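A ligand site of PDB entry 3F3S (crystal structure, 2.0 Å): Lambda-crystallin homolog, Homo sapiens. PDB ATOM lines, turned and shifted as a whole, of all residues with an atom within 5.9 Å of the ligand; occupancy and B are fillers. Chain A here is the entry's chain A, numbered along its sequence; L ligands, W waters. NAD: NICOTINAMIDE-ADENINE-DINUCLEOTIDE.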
ATOM      1  N   VAL A   9     -30.839  -9.475 -23.555  1.00  0.00           N
ATOM      2  CA  VAL A   9     -30.091  -8.908 -22.448  1.00  0.00           C
ATOM      3  C   VAL A   9     -28.873  -9.787 -22.204  1.00  0.00           C
ATOM      4  O   VAL A   9     -29.014 -10.881 -21.635  1.00  0.00           O
ATOM      5  CB  VAL A   9     -30.938  -8.836 -21.215  1.00  0.00           C
ATOM      6  CG1 VAL A   9     -30.091  -8.361 -19.989  1.00  0.00           C
ATOM      7  CG2 VAL A   9     -32.145  -7.909 -21.438  1.00  0.00           C
ATOM      8  N   GLY A  10     -27.711  -9.370 -22.670  1.00  0.00           N
ATOM      9  CA  GLY A  10     -26.517 -10.212 -22.636  1.00  0.00           C
ATOM     10  C   GLY A  10     -26.204 -10.705 -24.031  1.00  0.00           C
ATOM     11  O   GLY A  10     -26.810 -11.651 -24.516  1.00  0.00           O
ATOM     12  N   SER A  11     -25.254 -10.043 -24.676  1.00  0.00           N
ATOM     13  CA  SER A  11     -24.908 -10.353 -26.059  1.00  0.00           C
ATOM     14  C   SER A  11     -23.700 -11.271 -26.128  1.00  0.00           C
ATOM     15  O   SER A  11     -22.716 -10.985 -26.823  1.00  0.00           O
ATOM     16  CB  SER A  11     -24.656  -9.071 -26.857  1.00  0.00           C
ATOM     17  OG  SER A  11     -23.769  -8.209 -26.163  1.00  0.00           O
ATOM     18  N   GLY A  12     -23.794 -12.401 -25.427  1.00  0.00           N
ATOM     19  CA  GLY A  12     -22.739 -13.415 -25.441  1.00  0.00           C
ATOM     20  C   GLY A  12     -23.038 -14.554 -26.402  1.00  0.00           C
ATOM     21  O   GLY A  12     -23.635 -14.315 -27.433  1.00  0.00           O
ATOM     22  N   VAL A  13     -22.621 -15.771 -26.059  1.00  0.00           N
ATOM     23  CA  VAL A  13     -22.758 -16.940 -26.956  1.00  0.00           C
ATOM     24  C   VAL A  13     -24.231 -17.189 -27.259  1.00  0.00           C
ATOM     25  O   VAL A  13     -24.662 -17.237 -28.417  1.00  0.00           O
ATOM     26  CB  VAL A  13     -22.098 -18.210 -26.350  1.00  0.00           C
ATOM     27  CG1 VAL A  13     -22.401 -19.486 -27.194  1.00  0.00           C
ATOM     28  CG2 VAL A  13     -20.576 -18.014 -26.167  1.00  0.00           C
ATOM     29  N   ILE A  14     -25.029 -17.281 -26.212  1.00  0.00           N
ATOM     30  CA  ILE A  14     -26.410 -17.635 -26.363  1.00  0.00           C
ATOM     31  C   ILE A  14     -27.188 -16.453 -26.891  1.00  0.00           C
ATOM     32  O   ILE A  14     -28.018 -16.618 -27.789  1.00  0.00           O
ATOM     33  CB  ILE A  14     -26.989 -18.200 -25.025  1.00  0.00           C
ATOM     34  CG1 ILE A  14     -26.410 -19.591 -24.823  1.00  0.00           C
ATOM     35  CG2 ILE A  14     -28.536 -18.269 -25.034  1.00  0.00           C
ATOM     36  CD1 ILE A  14     -26.716 -20.645 -25.965  1.00  0.00           C
ATOM     37  N   GLY A  15     -26.893 -15.252 -26.392  1.00  0.00           N
ATOM     38  CA  GLY A  15     -27.538 -14.042 -26.921  1.00  0.00           C
ATOM     39  C   GLY A  15     -27.418 -13.844 -28.419  1.00  0.00           C
ATOM     40  O   GLY A  15     -28.401 -13.471 -29.097  1.00  0.00           O
ATOM     41  N   ARG A  16     -26.218 -14.036 -28.931  1.00  0.00           N
ATOM     42  CA  ARG A  16     -25.963 -13.935 -30.332  1.00  0.00           C
ATOM     43  C   ARG A  16     -26.767 -14.982 -31.121  1.00  0.00           C
ATOM     44  O   ARG A  16     -27.260 -14.658 -32.216  1.00  0.00           O
ATOM     45  CB  ARG A  16     -24.459 -14.100 -30.620  1.00  0.00           C
ATOM     46  CG  ARG A  16     -23.574 -12.888 -30.200  1.00  0.00           C
ATOM     47  CD  ARG A  16     -22.054 -13.227 -30.018  1.00  0.00           C
ATOM     48  NE  ARG A  16     -21.498 -12.216 -29.133  1.00  0.00           N
ATOM     49  CZ  ARG A  16     -20.224 -11.814 -29.071  1.00  0.00           C
ATOM     50  NH1 ARG A  16     -19.269 -12.374 -29.796  1.00  0.00           N
ATOM     51  NH2 ARG A  16     -19.914 -10.822 -28.215  1.00  0.00           N
ATOM     52  N   TYR A  32     -28.664  -5.759 -26.070  1.00  0.00           N
ATOM     53  CA  TYR A  32     -28.174  -4.995 -24.948  1.00  0.00           C
ATOM     54  C   TYR A  32     -27.137  -5.825 -24.167  1.00  0.00           C
ATOM     55  O   TYR A  32     -27.193  -7.046 -24.120  1.00  0.00           O
ATOM     56  CB  TYR A  32     -29.325  -4.579 -24.061  1.00  0.00           C
ATOM     57  CG  TYR A  32     -28.900  -4.071 -22.719  1.00  0.00           C
ATOM     58  CD1 TYR A  32     -28.423  -2.765 -22.552  1.00  0.00           C
ATOM     59  CD2 TYR A  32     -28.971  -4.891 -21.612  1.00  0.00           C
ATOM     60  CE1 TYR A  32     -28.014  -2.317 -21.297  1.00  0.00           C
ATOM     61  CE2 TYR A  32     -28.584  -4.444 -20.350  1.00  0.00           C
ATOM     62  CZ  TYR A  32     -28.112  -3.168 -20.194  1.00  0.00           C
ATOM     63  OH  TYR A  32     -27.728  -2.770 -18.946  1.00  0.00           O
ATOM     64  N   ASP A  33     -26.168  -5.134 -23.594  1.00  0.00           N
ATOM     65  CA  ASP A  33     -25.165  -5.743 -22.733  1.00  0.00           C
ATOM     66  C   ASP A  33     -24.700  -4.668 -21.755  1.00  0.00           C
ATOM     67  O   ASP A  33     -24.706  -3.463 -22.077  1.00  0.00           O
ATOM     68  CB  ASP A  33     -23.982  -6.268 -23.548  1.00  0.00           C
ATOM     69  CG  ASP A  33     -23.167  -7.326 -22.810  1.00  0.00           C
ATOM     70  OD1 ASP A  33     -22.337  -6.997 -21.925  1.00  0.00           O
ATOM     71  OD2 ASP A  33     -23.362  -8.526 -23.127  1.00  0.00           O
ATOM     72  N   ILE A  34     -24.247  -5.085 -20.588  1.00  0.00           N
ATOM     73  CA  ILE A  34     -23.712  -4.135 -19.633  1.00  0.00           C
ATOM     74  C   ILE A  34     -22.392  -3.556 -20.195  1.00  0.00           C
ATOM     75  O   ILE A  34     -22.022  -2.460 -19.859  1.00  0.00           O
ATOM     76  CB  ILE A  34     -23.559  -4.781 -18.226  1.00  0.00           C
ATOM     77  CG1 ILE A  34     -23.359  -3.704 -17.147  1.00  0.00           C
ATOM     78  CG2 ILE A  34     -22.410  -5.830 -18.249  1.00  0.00           C
ATOM     79  CD1 ILE A  34     -24.598  -2.854 -16.888  1.00  0.00           C
ATOM     80  N   GLU A  35     -21.700  -4.290 -21.072  1.00  0.00           N
ATOM     81  CA  GLU A  35     -20.479  -3.793 -21.740  1.00  0.00           C
ATOM     82  C   GLU A  35     -20.784  -3.493 -23.184  1.00  0.00           C
ATOM     83  O   GLU A  35     -21.114  -4.406 -23.958  1.00  0.00           O
ATOM     84  CB  GLU A  35     -19.387  -4.846 -21.751  1.00  0.00           C
ATOM     85  CG  GLU A  35     -18.803  -5.136 -20.421  1.00  0.00           C
ATOM     86  CD  GLU A  35     -17.757  -6.228 -20.460  1.00  0.00           C
ATOM     87  OE1 GLU A  35     -17.042  -6.345 -21.488  1.00  0.00           O
ATOM     88  OE2 GLU A  35     -17.647  -6.935 -19.447  1.00  0.00           O
ATOM     89  N   GLN A  38     -19.194  -5.427 -25.909  1.00  0.00           N
ATOM     90  CA  GLN A  38     -19.766  -6.727 -26.234  1.00  0.00           C
ATOM     91  C   GLN A  38     -20.910  -6.627 -27.267  1.00  0.00           C
ATOM     92  O   GLN A  38     -21.006  -7.461 -28.161  1.00  0.00           O
ATOM     93  CB  GLN A  38     -20.170  -7.494 -24.970  1.00  0.00           C
ATOM     94  CG  GLN A  38     -18.926  -7.940 -24.174  1.00  0.00           C
ATOM     95  CD  GLN A  38     -17.948  -8.770 -24.986  1.00  0.00           C
ATOM     96  OE1 GLN A  38     -18.322  -9.815 -25.479  1.00  0.00           O
ATOM     97  NE2 GLN A  38     -16.698  -8.313 -25.117  1.00  0.00           N
ATOM     98  N   GLU A  90     -33.250 -13.102 -21.569  1.00  0.00           N
ATOM     99  CA  GLU A  90     -32.069 -12.840 -20.736  1.00  0.00           C
ATOM    100  C   GLU A  90     -30.998 -13.930 -20.924  1.00  0.00           C
ATOM    101  O   GLU A  90     -31.275 -15.138 -20.845  1.00  0.00           O
ATOM    102  CB  GLU A  90     -32.499 -12.745 -19.277  1.00  0.00           C
ATOM    103  CG  GLU A  90     -31.337 -12.768 -18.283  1.00  0.00           C
ATOM    104  CD  GLU A  90     -30.911 -14.201 -17.911  1.00  0.00           C
ATOM    105  OE1 GLU A  90     -31.806 -14.982 -17.481  1.00  0.00           O
ATOM    106  OE2 GLU A  90     -29.719 -14.558 -18.097  1.00  0.00           O
ATOM    107  N   CYS A  91     -29.773 -13.479 -21.170  1.00  0.00           N
ATOM    108  CA  CYS A  91     -28.673 -14.355 -21.521  1.00  0.00           C
ATOM    109  C   CYS A  91     -27.405 -13.874 -20.849  1.00  0.00           C
ATOM    110  O   CYS A  91     -26.328 -13.802 -21.486  1.00  0.00           O
ATOM    111  CB  CYS A  91     -28.473 -14.343 -23.028  1.00  0.00           C
ATOM    112  SG  CYS A  91     -29.955 -14.606 -23.976  1.00  0.00           S
ATOM    113  N   VAL A  92     -27.546 -13.496 -19.587  1.00  0.00           N
ATOM    114  CA  VAL A  92     -26.376 -13.104 -18.815  1.00  0.00           C
ATOM    115  C   VAL A  92     -25.770 -14.337 -18.127  1.00  0.00           C
ATOM    116  O   VAL A  92     -26.332 -15.418 -18.194  1.00  0.00           O
ATOM    117  CB  VAL A  92     -26.728 -11.982 -17.828  1.00  0.00           C
ATOM    118  CG1 VAL A  92     -27.490 -10.871 -18.572  1.00  0.00           C
ATOM    119  CG2 VAL A  92     -27.537 -12.542 -16.616  1.00  0.00           C
ATOM    120  N   PRO A  93     -24.615 -14.175 -17.457  1.00  0.00           N
ATOM    121  CA  PRO A  93     -24.029 -15.365 -16.870  1.00  0.00           C
ATOM    122  C   PRO A  93     -24.911 -16.157 -15.913  1.00  0.00           C
ATOM    123  O   PRO A  93     -25.840 -15.633 -15.285  1.00  0.00           O
ATOM    124  CB  PRO A  93     -22.772 -14.838 -16.171  1.00  0.00           C
ATOM    125  CG  PRO A  93     -22.411 -13.623 -16.953  1.00  0.00           C
ATOM    126  CD  PRO A  93     -23.726 -13.005 -17.321  1.00  0.00           C
ATOM    127  N   GLU A  94     -24.612 -17.438 -15.809  1.00  0.00           N
ATOM    128  CA  GLU A  94     -25.380 -18.343 -14.943  1.00  0.00           C
ATOM    129  C   GLU A  94     -25.082 -18.073 -13.458  1.00  0.00           C
ATOM    130  O   GLU A  94     -24.314 -18.803 -12.840  1.00  0.00           O
ATOM    131  CB  GLU A  94     -25.044 -19.802 -15.306  1.00  0.00           C
ATOM    132  CG  GLU A  94     -25.955 -20.852 -14.620  1.00  0.00           C
ATOM    133  CD  GLU A  94     -27.271 -21.025 -15.344  1.00  0.00           C
ATOM    134  OE1 GLU A  94     -27.594 -22.200 -15.675  1.00  0.00           O
ATOM    135  OE2 GLU A  94     -27.958 -19.996 -15.598  1.00  0.00           O
ATOM    136  N   ASP A  95     -25.694 -17.037 -12.910  1.00  0.00           N
ATOM    137  CA  ASP A  95     -25.444 -16.584 -11.529  1.00  0.00           C
ATOM    138  C   ASP A  95     -26.740 -16.060 -10.967  1.00  0.00           C
ATOM    139  O   ASP A  95     -27.276 -15.075 -11.437  1.00  0.00           O
ATOM    140  CB  ASP A  95     -24.379 -15.466 -11.539  1.00  0.00           C
ATOM    141  CG  ASP A  95     -24.050 -14.931 -10.131  1.00  0.00           C
ATOM    142  OD1 ASP A  95     -22.918 -15.163  -9.694  1.00  0.00           O
ATOM    143  OD2 ASP A  95     -24.907 -14.310  -9.452  1.00  0.00           O
ATOM    144  N   LEU A  98     -26.977 -12.337  -9.745  1.00  0.00           N
ATOM    145  CA  LEU A  98     -26.916 -11.420 -10.903  1.00  0.00           C
ATOM    146  C   LEU A  98     -28.232 -11.414 -11.682  1.00  0.00           C
ATOM    147  O   LEU A  98     -28.719 -10.337 -12.068  1.00  0.00           O
ATOM    148  CB  LEU A  98     -25.760 -11.745 -11.871  1.00  0.00           C
ATOM    149  CG  LEU A  98     -25.716 -10.854 -13.140  1.00  0.00           C
ATOM    150  CD1 LEU A  98     -25.331  -9.401 -12.748  1.00  0.00           C
ATOM    151  CD2 LEU A  98     -24.755 -11.362 -14.173  1.00  0.00           C
ATOM    152  N   LYS A  99     -28.799 -12.594 -11.920  1.00  0.00           N
ATOM    153  CA  LYS A  99     -30.061 -12.680 -12.674  1.00  0.00           C
ATOM    154  C   LYS A  99     -31.206 -12.034 -11.913  1.00  0.00           C
ATOM    155  O   LYS A  99     -32.030 -11.332 -12.493  1.00  0.00           O
ATOM    156  CB  LYS A  99     -30.447 -14.134 -13.052  1.00  0.00           C
ATOM    157  CG  LYS A  99     -29.487 -14.776 -14.067  1.00  0.00           C
ATOM    158  CD  LYS A  99     -30.070 -15.975 -14.693  1.00  0.00           C
ATOM    159  CE  LYS A  99     -29.073 -16.818 -15.398  1.00  0.00           C
ATOM    160  NZ  LYS A  99     -28.418 -16.181 -16.567  1.00  0.00           N
ATOM    161  N   LYS A 101     -31.017  -9.641  -9.727  1.00  0.00           N
ATOM    162  CA  LYS A 101     -30.781  -8.188  -9.774  1.00  0.00           C
ATOM    163  C   LYS A 101     -31.319  -7.567 -11.065  1.00  0.00           C
ATOM    164  O   LYS A 101     -31.958  -6.522 -11.045  1.00  0.00           O
ATOM    165  CB  LYS A 101     -29.282  -7.911  -9.673  1.00  0.00           C
ATOM    166  CG  LYS A 101     -28.887  -6.452  -9.623  1.00  0.00           C
ATOM    167  CD  LYS A 101     -27.341  -6.266  -9.505  1.00  0.00           C
ATOM    168  CE  LYS A 101     -26.603  -6.512 -10.843  1.00  0.00           C
ATOM    169  NZ  LYS A 101     -25.101  -6.270 -10.776  1.00  0.00           N
ATOM    170  N   ILE A 102     -30.994  -8.188 -12.177  1.00  0.00           N
ATOM    171  CA  ILE A 102     -31.432  -7.712 -13.479  1.00  0.00           C
ATOM    172  C   ILE A 102     -32.926  -7.808 -13.569  1.00  0.00           C
ATOM    173  O   ILE A 102     -33.581  -6.883 -14.014  1.00  0.00           O
ATOM    174  CB  ILE A 102     -30.773  -8.492 -14.633  1.00  0.00           C
ATOM    175  CG1 ILE A 102     -29.271  -8.186 -14.672  1.00  0.00           C
ATOM    176  CG2 ILE A 102     -31.384  -8.083 -15.955  1.00  0.00           C
ATOM    177  CD1 ILE A 102     -28.485  -9.195 -15.426  1.00  0.00           C
ATOM    178  N   SER A 118     -35.896 -16.329 -19.270  1.00  0.00           N
ATOM    179  CA  SER A 118     -34.479 -16.645 -19.003  1.00  0.00           C
ATOM    180  C   SER A 118     -33.972 -17.831 -19.823  1.00  0.00           C
ATOM    181  O   SER A 118     -34.706 -18.791 -20.035  1.00  0.00           O
ATOM    182  CB  SER A 118     -34.260 -16.944 -17.518  1.00  0.00           C
ATOM    183  OG  SER A 118     -32.912 -17.315 -17.245  1.00  0.00           O
ATOM    184  N   SER A 119     -32.710 -17.758 -20.249  1.00  0.00           N
ATOM    185  CA  SER A 119     -32.028 -18.831 -20.950  1.00  0.00           C
ATOM    186  C   SER A 119     -31.382 -19.870 -20.035  1.00  0.00           C
ATOM    187  O   SER A 119     -30.701 -20.768 -20.527  1.00  0.00           O
ATOM    188  CB  SER A 119     -30.918 -18.270 -21.827  1.00  0.00           C
ATOM    189  OG  SER A 119     -31.446 -17.528 -22.894  1.00  0.00           O
ATOM    190  N   THR A 120     -31.603 -19.744 -18.731  1.00  0.00           N
ATOM    191  CA  THR A 120     -30.845 -20.504 -17.746  1.00  0.00           C
ATOM    192  C   THR A 120     -30.920 -21.996 -18.022  1.00  0.00           C
ATOM    193  O   THR A 120     -31.994 -22.545 -18.414  1.00  0.00           O
ATOM    194  CB  THR A 120     -31.361 -20.219 -16.313  1.00  0.00           C
ATOM    195  OG1 THR A 120     -30.541 -20.900 -15.366  1.00  0.00           O
ATOM    196  CG2 THR A 120     -32.790 -20.649 -16.147  1.00  0.00           C
ATOM    197  N   SER A 121     -29.812 -22.648 -17.778  1.00  0.00           N
ATOM    198  CA  SER A 121     -29.738 -24.101 -17.917  1.00  0.00           C
ATOM    199  C   SER A 121     -30.012 -24.797 -16.605  1.00  0.00           C
ATOM    200  O   SER A 121     -30.323 -25.986 -16.602  1.00  0.00           O
ATOM    201  CB  SER A 121     -28.398 -24.522 -18.472  1.00  0.00           C
ATOM    202  OG  SER A 121     -27.397 -24.451 -17.483  1.00  0.00           O
ATOM    203  N   CYS A 122     -29.923 -24.096 -15.480  1.00  0.00           N
ATOM    204  CA  CYS A 122     -30.118 -24.793 -14.201  1.00  0.00           C
ATOM    205  C   CYS A 122     -30.825 -24.055 -13.060  1.00  0.00           C
ATOM    206  O   CYS A 122     -31.108 -24.680 -12.053  1.00  0.00           O
ATOM    207  CB  CYS A 122     -28.789 -25.335 -13.716  1.00  0.00           C
ATOM    208  SG  CYS A 122     -27.805 -24.109 -12.835  1.00  0.00           S
ATOM    209  N   HIS A 142     -35.150 -22.401 -22.135  1.00  0.00           N
ATOM    210  CA  HIS A 142     -33.780 -22.906 -22.130  1.00  0.00           C
ATOM    211  C   HIS A 142     -33.454 -23.567 -23.468  1.00  0.00           C
ATOM    212  O   HIS A 142     -34.067 -24.591 -23.829  1.00  0.00           O
ATOM    213  CB  HIS A 142     -33.595 -23.920 -20.978  1.00  0.00           C
ATOM    214  CG  HIS A 142     -32.296 -24.673 -21.037  1.00  0.00           C
ATOM    215  ND1 HIS A 142     -32.240 -26.047 -21.165  1.00  0.00           N
ATOM    216  CD2 HIS A 142     -31.013 -24.239 -21.063  1.00  0.00           C
ATOM    217  CE1 HIS A 142     -30.973 -26.425 -21.245  1.00  0.00           C
ATOM    218  NE2 HIS A 142     -30.205 -25.352 -21.182  1.00  0.00           N
ATOM    219  N   PRO A 143     -32.496 -23.012 -24.213  1.00  0.00           N
ATOM    220  CA  PRO A 143     -32.098 -23.589 -25.475  1.00  0.00           C
ATOM    221  C   PRO A 143     -30.923 -24.574 -25.282  1.00  0.00           C
ATOM    222  O   PRO A 143     -30.428 -24.778 -24.178  1.00  0.00           O
ATOM    223  CB  PRO A 143     -31.646 -22.349 -26.259  1.00  0.00           C
ATOM    224  CG  PRO A 143     -30.967 -21.531 -25.162  1.00  0.00           C
ATOM    225  CD  PRO A 143     -31.793 -21.727 -23.958  1.00  0.00           C
ATOM    226  N   VAL A 144     -30.471 -25.191 -26.377  1.00  0.00           N
ATOM    227  CA  VAL A 144     -29.398 -26.173 -26.321  1.00  0.00           C
ATOM    228  C   VAL A 144     -28.312 -25.680 -27.236  1.00  0.00           C
ATOM    229  O   VAL A 144     -28.521 -25.461 -28.417  1.00  0.00           O
ATOM    230  CB  VAL A 144     -29.891 -27.569 -26.801  1.00  0.00           C
ATOM    231  CG1 VAL A 144     -28.773 -28.597 -26.765  1.00  0.00           C
ATOM    232  CG2 VAL A 144     -31.069 -28.042 -25.921  1.00  0.00           C
ATOM    233  N   ASN A 145     -27.101 -25.545 -26.719  1.00  0.00           N
ATOM    234  CA  ASN A 145     -26.046 -25.021 -27.573  1.00  0.00           C
ATOM    235  C   ASN A 145     -25.526 -26.117 -28.538  1.00  0.00           C
ATOM    236  O   ASN A 145     -25.350 -27.237 -28.108  1.00  0.00           O
ATOM    237  CB  ASN A 145     -24.893 -24.492 -26.704  1.00  0.00           C
ATOM    238  CG  ASN A 145     -23.921 -23.618 -27.491  1.00  0.00           C
ATOM    239  OD1 ASN A 145     -24.313 -22.618 -28.085  1.00  0.00           O
ATOM    240  ND2 ASN A 145     -22.677 -23.997 -27.493  1.00  0.00           N
HETATM  241  PA  NAD L   1     -21.714 -15.516 -21.899  1.00  0.00           P
HETATM  242  O1A NAD L   1     -20.771 -15.345 -20.777  1.00  0.00           O
HETATM  243  O2A NAD L   1     -21.363 -15.975 -23.231  1.00  0.00           O
HETATM  244  O5B NAD L   1     -22.477 -14.075 -22.170  1.00  0.00           O
HETATM  245  C5B NAD L   1     -23.028 -13.313 -21.065  1.00  0.00           C
HETATM  246  C4B NAD L   1     -23.214 -11.855 -21.457  1.00  0.00           C
HETATM  247  O4B NAD L   1     -23.853 -11.193 -20.318  1.00  0.00           O
HETATM  248  C3B NAD L   1     -21.818 -11.193 -21.628  1.00  0.00           C
HETATM  249  O3B NAD L   1     -21.711 -10.558 -22.924  1.00  0.00           O
HETATM  250  C2B NAD L   1     -21.751 -10.218 -20.444  1.00  0.00           C
HETATM  251  O2B NAD L   1     -21.078  -8.986 -20.775  1.00  0.00           O
HETATM  252  C1B NAD L   1     -23.237  -9.940 -20.233  1.00  0.00           C
HETATM  253  N9A NAD L   1     -23.525  -9.444 -18.930  1.00  0.00           N
HETATM  254  C8A NAD L   1     -22.925  -9.681 -17.764  1.00  0.00           C
HETATM  255  N7A NAD L   1     -23.581  -9.008 -16.788  1.00  0.00           N
HETATM  256  C5A NAD L   1     -24.582  -8.327 -17.353  1.00  0.00           C
HETATM  257  C6A NAD L   1     -25.593  -7.462 -16.895  1.00  0.00           C
HETATM  258  N6A NAD L   1     -25.720  -7.075 -15.617  1.00  0.00           N
HETATM  259  N1A NAD L   1     -26.454  -6.993 -17.779  1.00  0.00           N
HETATM  260  C2A NAD L   1     -26.401  -7.291 -19.074  1.00  0.00           C
HETATM  261  N3A NAD L   1     -25.457  -8.087 -19.546  1.00  0.00           N
HETATM  262  C4A NAD L   1     -24.535  -8.606 -18.711  1.00  0.00           C
HETATM  263  O3  NAD L   1     -22.945 -16.498 -21.318  1.00  0.00           O
HETATM  264  PN  NAD L   1     -23.660 -17.518 -22.273  1.00  0.00           P
HETATM  265  O1N NAD L   1     -22.901 -18.755 -22.467  1.00  0.00           O
HETATM  266  O2N NAD L   1     -24.200 -16.908 -23.480  1.00  0.00           O
HETATM  267  O5D NAD L   1     -24.853 -17.966 -21.212  1.00  0.00           O
HETATM  268  C5D NAD L   1     -25.862 -17.085 -20.865  1.00  0.00           C
HETATM  269  C4D NAD L   1     -27.017 -17.900 -20.217  1.00  0.00           C
HETATM  270  O4D NAD L   1     -27.405 -18.952 -21.182  1.00  0.00           O
HETATM  271  C3D NAD L   1     -26.603 -18.598 -18.925  1.00  0.00           C
HETATM  272  O3D NAD L   1     -27.700 -18.627 -17.933  1.00  0.00           O
HETATM  273  C2D NAD L   1     -26.325 -19.989 -19.365  1.00  0.00           C
HETATM  274  O2D NAD L   1     -26.574 -20.903 -18.302  1.00  0.00           O
HETATM  275  C1D NAD L   1     -27.410 -20.159 -20.476  1.00  0.00           C
HETATM  276  N1N NAD L   1     -27.105 -21.195 -21.438  1.00  0.00           N
HETATM  277  C2N NAD L   1     -25.789 -21.299 -21.957  1.00  0.00           C
HETATM  278  C3N NAD L   1     -25.508 -22.303 -22.866  1.00  0.00           C
HETATM  279  C7N NAD L   1     -24.064 -22.409 -23.397  1.00  0.00           C
HETATM  280  O7N NAD L   1     -23.274 -21.459 -23.392  1.00  0.00           O
HETATM  281  N7N NAD L   1     -23.787 -23.576 -23.927  1.00  0.00           N
HETATM  282  C4N NAD L   1     -26.521 -23.195 -23.317  1.00  0.00           C
HETATM  283  C5N NAD L   1     -27.816 -23.062 -22.857  1.00  0.00           C
HETATM  284  C6N NAD L   1     -28.104 -22.084 -21.903  1.00  0.00           C
HETATM  285  O   HOH W   1     -27.832  -4.558 -17.043  1.00  0.00           O
HETATM  286  O   HOH W   2     -22.093  -8.308 -14.353  1.00  0.00           O
HETATM  287  O   HOH W   3     -22.630 -20.569 -19.773  1.00  0.00           O
HETATM  288  O   HOH W   4     -19.966 -11.506 -24.590  1.00  0.00           O
HETATM  289  O   HOH W   5     -20.732 -16.890 -18.602  1.00  0.00           O
HETATM  290  O   HOH W   6     -19.668  -7.926 -17.972  1.00  0.00           O
HETATM  291  O   HOH W   7     -20.686 -21.993 -24.570  1.00  0.00           O
HETATM  292  O   HOH W   8     -20.265 -19.369 -22.961  1.00  0.00           O
HETATM  293  O   HOH W   9     -25.359 -14.522 -24.095  1.00  0.00           O
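Water W4 lies within hydrogen-bond range of the side-chain amide oxygen of Gln 38 and an oxygen (O3B) of the ligand. Water W1 lies within hydrogen-bond range of the side-chain hydroxyl (OH) of Tyr 32 (2.6 Å) and a nitrogen (N1A) of the ligand (2.9 Å). Water W6 lies within hydrogen-bond range of OE2 of Glu 35 (2.7 Å) and O2B of the ligand (3.3 Å).
The backbone NH (N) of Glu 35 sits at hydrogen-bond distance from the side-chain carboxylate (OD1) of Asp 33 (2.9 Å). The side-chain carboxylate (OE2) of Glu 94 lies within hydrogen-bond range of the side-chain hydroxyl (OG1) of Thr 120 (2.7 Å). OE1 of Glu 94 lies within hydrogen-bond range of OG of Ser 121 (2.9 Å). N of Val 92 is in hydrogen-bond range of OE2 of Glu 90. The backbone NH of Cys 122 is in hydrogen-bond range of the side-chain hydroxyl of Thr 120, 3.3 Å away. OD2 of Asp 95 is in hydrogen-bond range of N of Leu 98 (2.9 Å). The guanidinium group (NE) of Arg 16 sits at hydrogen-bond distance from the backbone carbonyl oxygen (O) of Ser 11, at 2.9 Å. OE1 of Gln 38 lies within hydrogen-bond range of NH2 of Arg 16 (3.3 Å).
Residues that only touch the ligand: Asn 145 (3.1 Å), Ser 119 (3.2 Å), Gly 12 (3.3 Å), Cys 91 (3.4 Å), Pro 143 (3.4 Å), Pro 93 (3.4 Å), Ile 102 (3.5 Å), Gly 10 (3.7 Å), Thr 120 (3.7 Å), His 142 (3.7 Å), Leu 98 (3.7 Å), Ser 121 (3.7 Å), Tyr 32 (3.8 Å), Ser 11 (3.8 Å), Val 9 (3.9 Å) and Gln 38 (3.99 Å). Hydrophobic or aromatic side chains that line the ligand: Val 9, Val 13, Ile 14, Tyr 32, Ile 34, Val 92, Pro 93, Leu 98, Ile 102 and His 142. 23 residues have an atom within 4 Å of the ligand: Val 9, Gly 10, Ser 11, Gly 12, Val 13, Ile 14, Tyr 32, Asp 33, Ile 34, Gln 38, Cys 91, Val 92, Pro 93, Glu 94, Leu 98, Lys 99, Ile 102, Ser 119, Thr 120, Ser 121, His 142, Pro 143 and Asn 145.
O2B of the ligand lies within hydrogen-bond range of OD1 of Asp 33 (2.6 Å). The side-chain carboxylate (OE2) of Glu 94 lies within hydrogen-bond range of an oxygen (O3D) of the ligand (2.7 Å). N of Ile 14 is in hydrogen-bond range of O2N of the ligand, 2.9 Å away. NZ of Lys 99 is in hydrogen-bond range of O3D of the ligand, at 2.9 Å. The backbone NH of Val 13 sits at hydrogen-bond distance from an oxygen (O2A) of the ligand. O3D of the ligand lies close to O of Val 92. A nitrogen (N3A) of the ligand is in hydrogen-bond range of the backbone NH (N) of Ile 34 (3.4 Å).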
